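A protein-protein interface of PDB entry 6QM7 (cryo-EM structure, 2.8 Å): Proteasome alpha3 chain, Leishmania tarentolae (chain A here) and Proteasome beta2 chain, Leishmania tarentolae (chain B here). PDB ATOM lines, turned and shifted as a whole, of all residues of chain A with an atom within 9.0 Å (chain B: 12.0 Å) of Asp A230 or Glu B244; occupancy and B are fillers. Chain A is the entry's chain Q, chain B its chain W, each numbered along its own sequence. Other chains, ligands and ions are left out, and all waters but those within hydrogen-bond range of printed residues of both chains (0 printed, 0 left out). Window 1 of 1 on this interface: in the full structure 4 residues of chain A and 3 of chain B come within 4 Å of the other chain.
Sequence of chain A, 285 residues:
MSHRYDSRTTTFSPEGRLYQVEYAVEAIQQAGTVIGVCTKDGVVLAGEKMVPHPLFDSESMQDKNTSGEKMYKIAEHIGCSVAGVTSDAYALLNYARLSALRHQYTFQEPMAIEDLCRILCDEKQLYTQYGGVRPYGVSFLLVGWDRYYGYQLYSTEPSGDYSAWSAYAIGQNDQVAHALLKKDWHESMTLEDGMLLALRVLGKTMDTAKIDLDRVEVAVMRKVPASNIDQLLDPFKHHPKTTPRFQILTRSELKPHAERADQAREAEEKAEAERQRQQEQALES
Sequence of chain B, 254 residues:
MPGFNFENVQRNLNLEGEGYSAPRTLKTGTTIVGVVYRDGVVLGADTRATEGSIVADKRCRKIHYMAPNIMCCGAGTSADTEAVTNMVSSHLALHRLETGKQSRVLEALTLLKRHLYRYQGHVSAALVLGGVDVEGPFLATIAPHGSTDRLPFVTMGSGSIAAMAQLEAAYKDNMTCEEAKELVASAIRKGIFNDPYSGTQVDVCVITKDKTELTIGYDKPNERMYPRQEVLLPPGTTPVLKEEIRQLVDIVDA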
ATOM      1  N   ALA A 226      17.915  12.617  17.980  1.00  0.00           N
ATOM      2  CA  ALA A 226      17.168  12.482  19.253  1.00  0.00           C
ATOM      3  C   ALA A 226      17.120  11.002  19.637  1.00  0.00           C
ATOM      4  O   ALA A 226      16.707  10.195  18.784  1.00  0.00           O
ATOM      5  CB  ALA A 226      15.784  13.061  19.110  1.00  0.00           C
ATOM      6  N   SER A 227      17.518  10.676  20.873  1.00  0.00           N
ATOM      7  CA  SER A 227      17.745   9.293  21.376  1.00  0.00           C
ATOM      8  C   SER A 227      16.611   8.865  22.319  1.00  0.00           C
ATOM      9  O   SER A 227      15.960   7.839  22.022  1.00  0.00           O
ATOM     10  CB  SER A 227      19.101   9.177  22.040  1.00  0.00           C
ATOM     11  OG  SER A 227      19.314  10.239  22.959  1.00  0.00           O
ATOM     12  N   ASN A 228      16.396   9.611  23.411  1.00  0.00           N
ATOM     13  CA  ASN A 228      15.374   9.304  24.455  1.00  0.00           C
ATOM     14  C   ASN A 228      13.994   9.734  23.934  1.00  0.00           C
ATOM     15  O   ASN A 228      13.489  10.797  24.351  1.00  0.00           O
ATOM     16  CB  ASN A 228      15.730   9.894  25.831  1.00  0.00           C
ATOM     17  CG  ASN A 228      15.982  11.389  25.839  1.00  0.00           C
ATOM     18  OD1 ASN A 228      16.208  11.999  24.795  1.00  0.00           O
ATOM     19  ND2 ASN A 228      15.955  11.989  27.018  1.00  0.00           N
ATOM     20  N   ILE A 229      13.407   8.912  23.059  1.00  0.00           N
ATOM     21  CA  ILE A 229      12.069   9.146  22.436  1.00  0.00           C
ATOM     22  C   ILE A 229      11.011   8.887  23.524  1.00  0.00           C
ATOM     23  O   ILE A 229      10.260   9.831  23.848  1.00  0.00           O
ATOM     24  CB  ILE A 229      11.856   8.263  21.177  1.00  0.00           C
ATOM     25  CG1 ILE A 229      13.018   8.324  20.174  1.00  0.00           C
ATOM     26  CG2 ILE A 229      10.539   8.596  20.493  1.00  0.00           C
ATOM     27  CD1 ILE A 229      13.144   9.634  19.427  1.00  0.00           C
ATOM     28  N   ASP A 230      11.003   7.668  24.089  1.00  0.00           N
ATOM     29  CA  ASP A 230      10.006   7.135  25.066  1.00  0.00           C
ATOM     30  C   ASP A 230       8.607   7.203  24.433  1.00  0.00           C
ATOM     31  O   ASP A 230       7.689   7.755  25.075  1.00  0.00           O
ATOM     32  CB  ASP A 230      10.090   7.849  26.427  1.00  0.00           C
ATOM     33  CG  ASP A 230      11.350   7.568  27.242  1.00  0.00           C
ATOM     34  OD1 ASP A 230      11.848   6.424  27.197  1.00  0.00           O
ATOM     35  OD2 ASP A 230      11.819   8.498  27.933  1.00  0.00           O
ATOM     36  N   GLN A 231       8.459   6.643  23.224  1.00  0.00           N
ATOM     37  CA  GLN A 231       7.236   6.742  22.380  1.00  0.00           C
ATOM     38  C   GLN A 231       6.055   6.040  23.064  1.00  0.00           C
ATOM     39  O   GLN A 231       4.919   6.499  22.862  1.00  0.00           O
ATOM     40  CB  GLN A 231       7.469   6.144  20.986  1.00  0.00           C
ATOM     41  CG  GLN A 231       6.339   6.389  19.980  1.00  0.00           C
ATOM     42  CD  GLN A 231       6.145   7.840  19.593  1.00  0.00           C
ATOM     43  OE1 GLN A 231       6.951   8.423  18.869  1.00  0.00           O
ATOM     44  NE2 GLN A 231       5.058   8.438  20.054  1.00  0.00           N
ATOM     45  N   LEU A 232       6.291   4.977  23.839  1.00  0.00           N
ATOM     46  CA  LEU A 232       5.190   4.168  24.425  1.00  0.00           C
ATOM     47  C   LEU A 232       4.493   4.939  25.548  1.00  0.00           C
ATOM     48  O   LEU A 232       3.359   4.546  25.876  1.00  0.00           O
ATOM     49  CB  LEU A 232       5.725   2.832  24.941  1.00  0.00           C
ATOM     50  CG  LEU A 232       6.279   1.890  23.874  1.00  0.00           C
ATOM     51  CD1 LEU A 232       6.762   0.595  24.506  1.00  0.00           C
ATOM     52  CD2 LEU A 232       5.244   1.606  22.802  1.00  0.00           C
ATOM     53  N   LEU A 233       5.129   5.968  26.117  1.00  0.00           N
ATOM     54  CA  LEU A 233       4.578   6.729  27.272  1.00  0.00           C
ATOM     55  C   LEU A 233       3.573   7.780  26.796  1.00  0.00           C
ATOM     56  O   LEU A 233       2.633   8.077  27.571  1.00  0.00           O
ATOM     57  CB  LEU A 233       5.708   7.391  28.058  1.00  0.00           C
ATOM     58  CG  LEU A 233       6.686   6.454  28.758  1.00  0.00           C
ATOM     59  CD1 LEU A 233       7.493   7.226  29.776  1.00  0.00           C
ATOM     60  CD2 LEU A 233       5.983   5.295  29.431  1.00  0.00           C
ATOM     61  N   ASP A 234       3.770   8.345  25.601  1.00  0.00           N
ATOM     62  CA  ASP A 234       2.742   9.162  24.901  1.00  0.00           C
ATOM     63  C   ASP A 234       2.681   8.712  23.441  1.00  0.00           C
ATOM     64  O   ASP A 234       3.412   9.226  22.603  1.00  0.00           O
ATOM     65  CB  ASP A 234       3.011  10.655  25.110  1.00  0.00           C
ATOM     66  CG  ASP A 234       1.748  11.513  25.102  1.00  0.00           C
ATOM     67  OD1 ASP A 234       0.804  11.177  24.340  1.00  0.00           O
ATOM     68  OD2 ASP A 234       1.708  12.507  25.870  1.00  0.00           O
ATOM     69  N   PRO A 235       1.834   7.717  23.099  1.00  0.00           N
ATOM     70  CA  PRO A 235       1.761   7.184  21.736  1.00  0.00           C
ATOM     71  C   PRO A 235       1.471   8.204  20.622  1.00  0.00           C
ATOM     72  O   PRO A 235       1.884   7.976  19.502  1.00  0.00           O
ATOM     73  CB  PRO A 235       0.573   6.206  21.782  1.00  0.00           C
ATOM     74  CG  PRO A 235       0.454   5.815  23.238  1.00  0.00           C
ATOM     75  CD  PRO A 235       0.919   7.023  24.018  1.00  0.00           C
ATOM     76  N   PHE A 236       0.745   9.271  20.952  1.00  0.00           N
ATOM     77  CA  PHE A 236       0.227  10.269  19.989  1.00  0.00           C
ATOM     78  C   PHE A 236       1.205  11.435  19.842  1.00  0.00           C
ATOM     79  O   PHE A 236       1.010  12.241  18.920  1.00  0.00           O
ATOM     80  CB  PHE A 236      -1.157  10.732  20.437  1.00  0.00           C
ATOM     81  CG  PHE A 236      -2.200   9.649  20.347  1.00  0.00           C
ATOM     82  CD1 PHE A 236      -2.846   9.384  19.149  1.00  0.00           C
ATOM     83  CD2 PHE A 236      -2.517   8.881  21.458  1.00  0.00           C
ATOM     84  CE1 PHE A 236      -3.798   8.379  19.067  1.00  0.00           C
ATOM     85  CE2 PHE A 236      -3.465   7.873  21.375  1.00  0.00           C
ATOM     86  CZ  PHE A 236      -4.103   7.622  20.179  1.00  0.00           C
ATOM     87  N   LYS A 237       2.214  11.527  20.706  1.00  0.00           N
ATOM     88  CA  LYS A 237       3.196  12.639  20.689  1.00  0.00           C
ATOM     89  C   LYS A 237       4.189  12.347  19.566  1.00  0.00           C
ATOM     90  O   LYS A 237       4.729  11.229  19.536  1.00  0.00           O
ATOM     91  CB  LYS A 237       3.860  12.804  22.063  1.00  0.00           C
ATOM     92  CG  LYS A 237       4.179  14.240  22.475  1.00  0.00           C
ATOM     93  CD  LYS A 237       5.653  14.616  22.363  1.00  0.00           C
ATOM     94  CE  LYS A 237       5.900  16.109  22.260  1.00  0.00           C
ATOM     95  NZ  LYS A 237       5.569  16.810  23.524  1.00  0.00           N
ATOM     96  N   HIS A 239       7.730  12.902  18.089  1.00  0.00           N
ATOM     97  CA  HIS A 239       9.126  13.240  18.454  1.00  0.00           C
ATOM     98  C   HIS A 239       9.905  13.461  17.161  1.00  0.00           C
ATOM     99  O   HIS A 239       9.944  12.566  16.313  1.00  0.00           O
ATOM    100  CB  HIS A 239       9.708  12.159  19.362  1.00  0.00           C
ATOM    101  CG  HIS A 239       8.919  11.975  20.611  1.00  0.00           C
ATOM    102  ND1 HIS A 239       8.971  12.879  21.657  1.00  0.00           N
ATOM    103  CD2 HIS A 239       8.047  11.011  20.978  1.00  0.00           C
ATOM    104  CE1 HIS A 239       8.167  12.472  22.621  1.00  0.00           C
ATOM    105  NE2 HIS A 239       7.586  11.326  22.229  1.00  0.00           N
ATOM    106  N   VAL B 240       3.743  -9.476  25.959  1.00  0.00           N
ATOM    107  CA  VAL B 240       4.279  -8.109  25.720  1.00  0.00           C
ATOM    108  C   VAL B 240       4.106  -7.763  24.239  1.00  0.00           C
ATOM    109  O   VAL B 240       4.694  -8.467  23.396  1.00  0.00           O
ATOM    110  CB  VAL B 240       5.751  -8.043  26.157  1.00  0.00           C
ATOM    111  CG1 VAL B 240       6.459  -6.798  25.636  1.00  0.00           C
ATOM    112  CG2 VAL B 240       5.868  -8.143  27.669  1.00  0.00           C
ATOM    113  N   LEU B 241       3.359  -6.698  23.950  1.00  0.00           N
ATOM    114  CA  LEU B 241       3.064  -6.231  22.575  1.00  0.00           C
ATOM    115  C   LEU B 241       4.301  -5.539  21.994  1.00  0.00           C
ATOM    116  O   LEU B 241       4.749  -5.954  20.906  1.00  0.00           O
ATOM    117  CB  LEU B 241       1.865  -5.281  22.610  1.00  0.00           C
ATOM    118  CG  LEU B 241       0.562  -5.901  23.111  1.00  0.00           C
ATOM    119  CD1 LEU B 241      -0.534  -4.846  23.204  1.00  0.00           C
ATOM    120  CD2 LEU B 241       0.131  -7.065  22.221  1.00  0.00           C
ATOM    121  N   LYS B 242       4.816  -4.522  22.687  1.00  0.00           N
ATOM    122  CA  LYS B 242       5.986  -3.716  22.245  1.00  0.00           C
ATOM    123  C   LYS B 242       7.010  -3.618  23.374  1.00  0.00           C
ATOM    124  O   LYS B 242       6.643  -3.822  24.537  1.00  0.00           O
ATOM    125  CB  LYS B 242       5.557  -2.315  21.804  1.00  0.00           C
ATOM    126  CG  LYS B 242       4.968  -2.249  20.404  1.00  0.00           C
ATOM    127  CD  LYS B 242       4.165  -0.988  20.127  1.00  0.00           C
ATOM    128  CE  LYS B 242       2.921  -1.254  19.301  1.00  0.00           C
ATOM    129  NZ  LYS B 242       1.994  -0.100  19.327  1.00  0.00           N
ATOM    130  N   GLU B 243       8.247  -3.306  23.005  1.00  0.00           N
ATOM    131  CA  GLU B 243       9.406  -3.215  23.922  1.00  0.00           C
ATOM    132  C   GLU B 243      10.402  -2.221  23.325  1.00  0.00           C
ATOM    133  O   GLU B 243      10.831  -2.449  22.186  1.00  0.00           O
ATOM    134  CB  GLU B 243      10.007  -4.608  24.114  1.00  0.00           C
ATOM    135  CG  GLU B 243      11.198  -4.645  25.054  1.00  0.00           C
ATOM    136  CD  GLU B 243      11.731  -6.037  25.365  1.00  0.00           C
ATOM    137  OE1 GLU B 243      10.913  -6.978  25.517  1.00  0.00           O
ATOM    138  OE2 GLU B 243      12.968  -6.177  25.479  1.00  0.00           O
ATOM    139  N   GLU B 244      10.704  -1.145  24.045  1.00  0.00           N
ATOM    140  CA  GLU B 244      11.797  -0.195  23.720  1.00  0.00           C
ATOM    141  C   GLU B 244      12.864  -0.321  24.807  1.00  0.00           C
ATOM    142  O   GLU B 244      12.566   0.051  25.956  1.00  0.00           O
ATOM    143  CB  GLU B 244      11.281   1.244  23.656  1.00  0.00           C
ATOM    144  CG  GLU B 244      10.399   1.533  22.454  1.00  0.00           C
ATOM    145  CD  GLU B 244       9.785   2.930  22.400  1.00  0.00           C
ATOM    146  OE1 GLU B 244       9.881   3.680  23.405  1.00  0.00           O
ATOM    147  OE2 GLU B 244       9.199   3.264  21.346  1.00  0.00           O
ATOM    148  N   ILE B 245      14.049  -0.821  24.453  1.00  0.00           N
ATOM    149  CA  ILE B 245      15.256  -0.801  25.329  1.00  0.00           C
ATOM    150  C   ILE B 245      16.066   0.456  25.003  1.00  0.00           C
ATOM    151  O   ILE B 245      16.191   0.782  23.820  1.00  0.00           O
ATOM    152  CB  ILE B 245      16.090  -2.086  25.172  1.00  0.00           C
ATOM    153  CG1 ILE B 245      15.262  -3.342  25.482  1.00  0.00           C
ATOM    154  CG2 ILE B 245      17.347  -2.000  26.031  1.00  0.00           C
ATOM    155  CD1 ILE B 245      15.944  -4.652  25.135  1.00  0.00           C
ATOM    156  N   ARG B 246      16.556   1.145  26.033  1.00  0.00           N
ATOM    157  CA  ARG B 246      17.483   2.300  25.915  1.00  0.00           C
ATOM    158  C   ARG B 246      18.673   2.052  26.846  1.00  0.00           C
ATOM    159  O   ARG B 246      18.436   1.893  28.058  1.00  0.00           O
ATOM    160  CB  ARG B 246      16.769   3.607  26.267  1.00  0.00           C
ATOM    161  CG  ARG B 246      17.512   4.853  25.809  1.00  0.00           C
ATOM    162  CD  ARG B 246      16.779   6.138  26.149  1.00  0.00           C
ATOM    163  NE  ARG B 246      17.117   6.638  27.482  1.00  0.00           N
ATOM    164  CZ  ARG B 246      16.274   6.826  28.505  1.00  0.00           C
ATOM    165  NH1 ARG B 246      14.977   6.565  28.405  1.00  0.00           N
ATOM    166  NH2 ARG B 246      16.748   7.292  29.649  1.00  0.00           N
ATOM    167  N   GLN B 247      19.890   1.993  26.293  1.00  0.00           N
ATOM    168  CA  GLN B 247      21.162   1.846  27.051  1.00  0.00           C
ATOM    169  C   GLN B 247      21.644   3.237  27.497  1.00  0.00           C
ATOM    170  O   GLN B 247      21.307   4.231  26.812  1.00  0.00           O
ATOM    171  CB  GLN B 247      22.219   1.144  26.190  1.00  0.00           C
ATOM    172  CG  GLN B 247      21.827  -0.258  25.727  1.00  0.00           C
ATOM    173  CD  GLN B 247      21.856  -1.317  26.805  1.00  0.00           C
ATOM    174  OE1 GLN B 247      21.223  -2.364  26.675  1.00  0.00           O
ATOM    175  NE2 GLN B 247      22.598  -1.070  27.877  1.00  0.00           N
ATOM    176  N   LEU B 248      22.414   3.293  28.593  1.00  0.00           N
ATOM    177  CA  LEU B 248      22.972   4.536  29.201  1.00  0.00           C
ATOM    178  C   LEU B 248      24.500   4.399  29.325  1.00  0.00           C
ATOM    179  O   LEU B 248      25.287   4.943  28.539  1.00  0.00           O
ATOM    180  CB  LEU B 248      22.318   4.763  30.572  1.00  0.00           C
ATOM    181  CG  LEU B 248      20.800   4.555  30.657  1.00  0.00           C
ATOM    182  CD1 LEU B 248      20.325   4.521  32.107  1.00  0.00           C
ATOM    183  CD2 LEU B 248      20.049   5.626  29.877  1.00  0.00           C
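The guanidinium group (NH1) of Arg B246 lies within salt-bridge range of the side-chain carboxylate (OD1) of Asp A230 (3.4 Å).
The backbone NH (N) of Gln A231 sits at hydrogen-bond distance from the side-chain carboxylate (OE1) of Glu B244 (3.3 Å).
O of Asp A234 is in hydrogen-bond range of NE2 of Gln A231, at 3.1 Å.
The side-chain amide nitrogen (NE2) of Gln A231 sits at hydrogen-bond distance from the backbone carbonyl oxygen (O) of Pro A235.
The backbone carbonyl oxygen (O) of Lys A237 is in hydrogen-bond range of the side-chain amide nitrogen (NE2) of Gln A231, at 2.9 Å.
Among the printed residues, merely in contact across the chains: Asp A230 with Glu B244 (3.8 Å), Leu A232 with Glu B244 (3.8 Å), Asn A228 with Arg B246 (3.9 Å) and Leu A232 with Lys B242 (3.9 Å).
Glu B244 touches three residues of chain A.
Of the printed residues of chain B, Asn A228 touches Arg B246.
No residue of chain B comes within 4 Å of Ile A229.
No residue of chain B comes within 4 Å of Leu A233.
No residue of chain B comes within 4 Å of Asp A234.
Of the printed residues of chain A, Lys B242 touches Leu A232.
Printed residues of chain A within 4 Å of Arg B246: Asn A228 and Asp A230.
The nearest printed residue of chain A that does not touch Arg B246 is Ser A227 (4.5 Å).
Of the 13 printed residues of chain A, 4 touch a printed residue of chain B.
Printed residues of chain A that touch a printed residue of chain B: Asn A228, Asp A230, Gln A231 and Leu A232.
Among the printed residues, 6 pairs touch across the chains.
Among the printed residues, Asp or Glu carboxylates within 4 Å of a Lys or Arg side-chain nitrogen of the other chain: Asp A230 with Arg B246 (3.4 Å).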
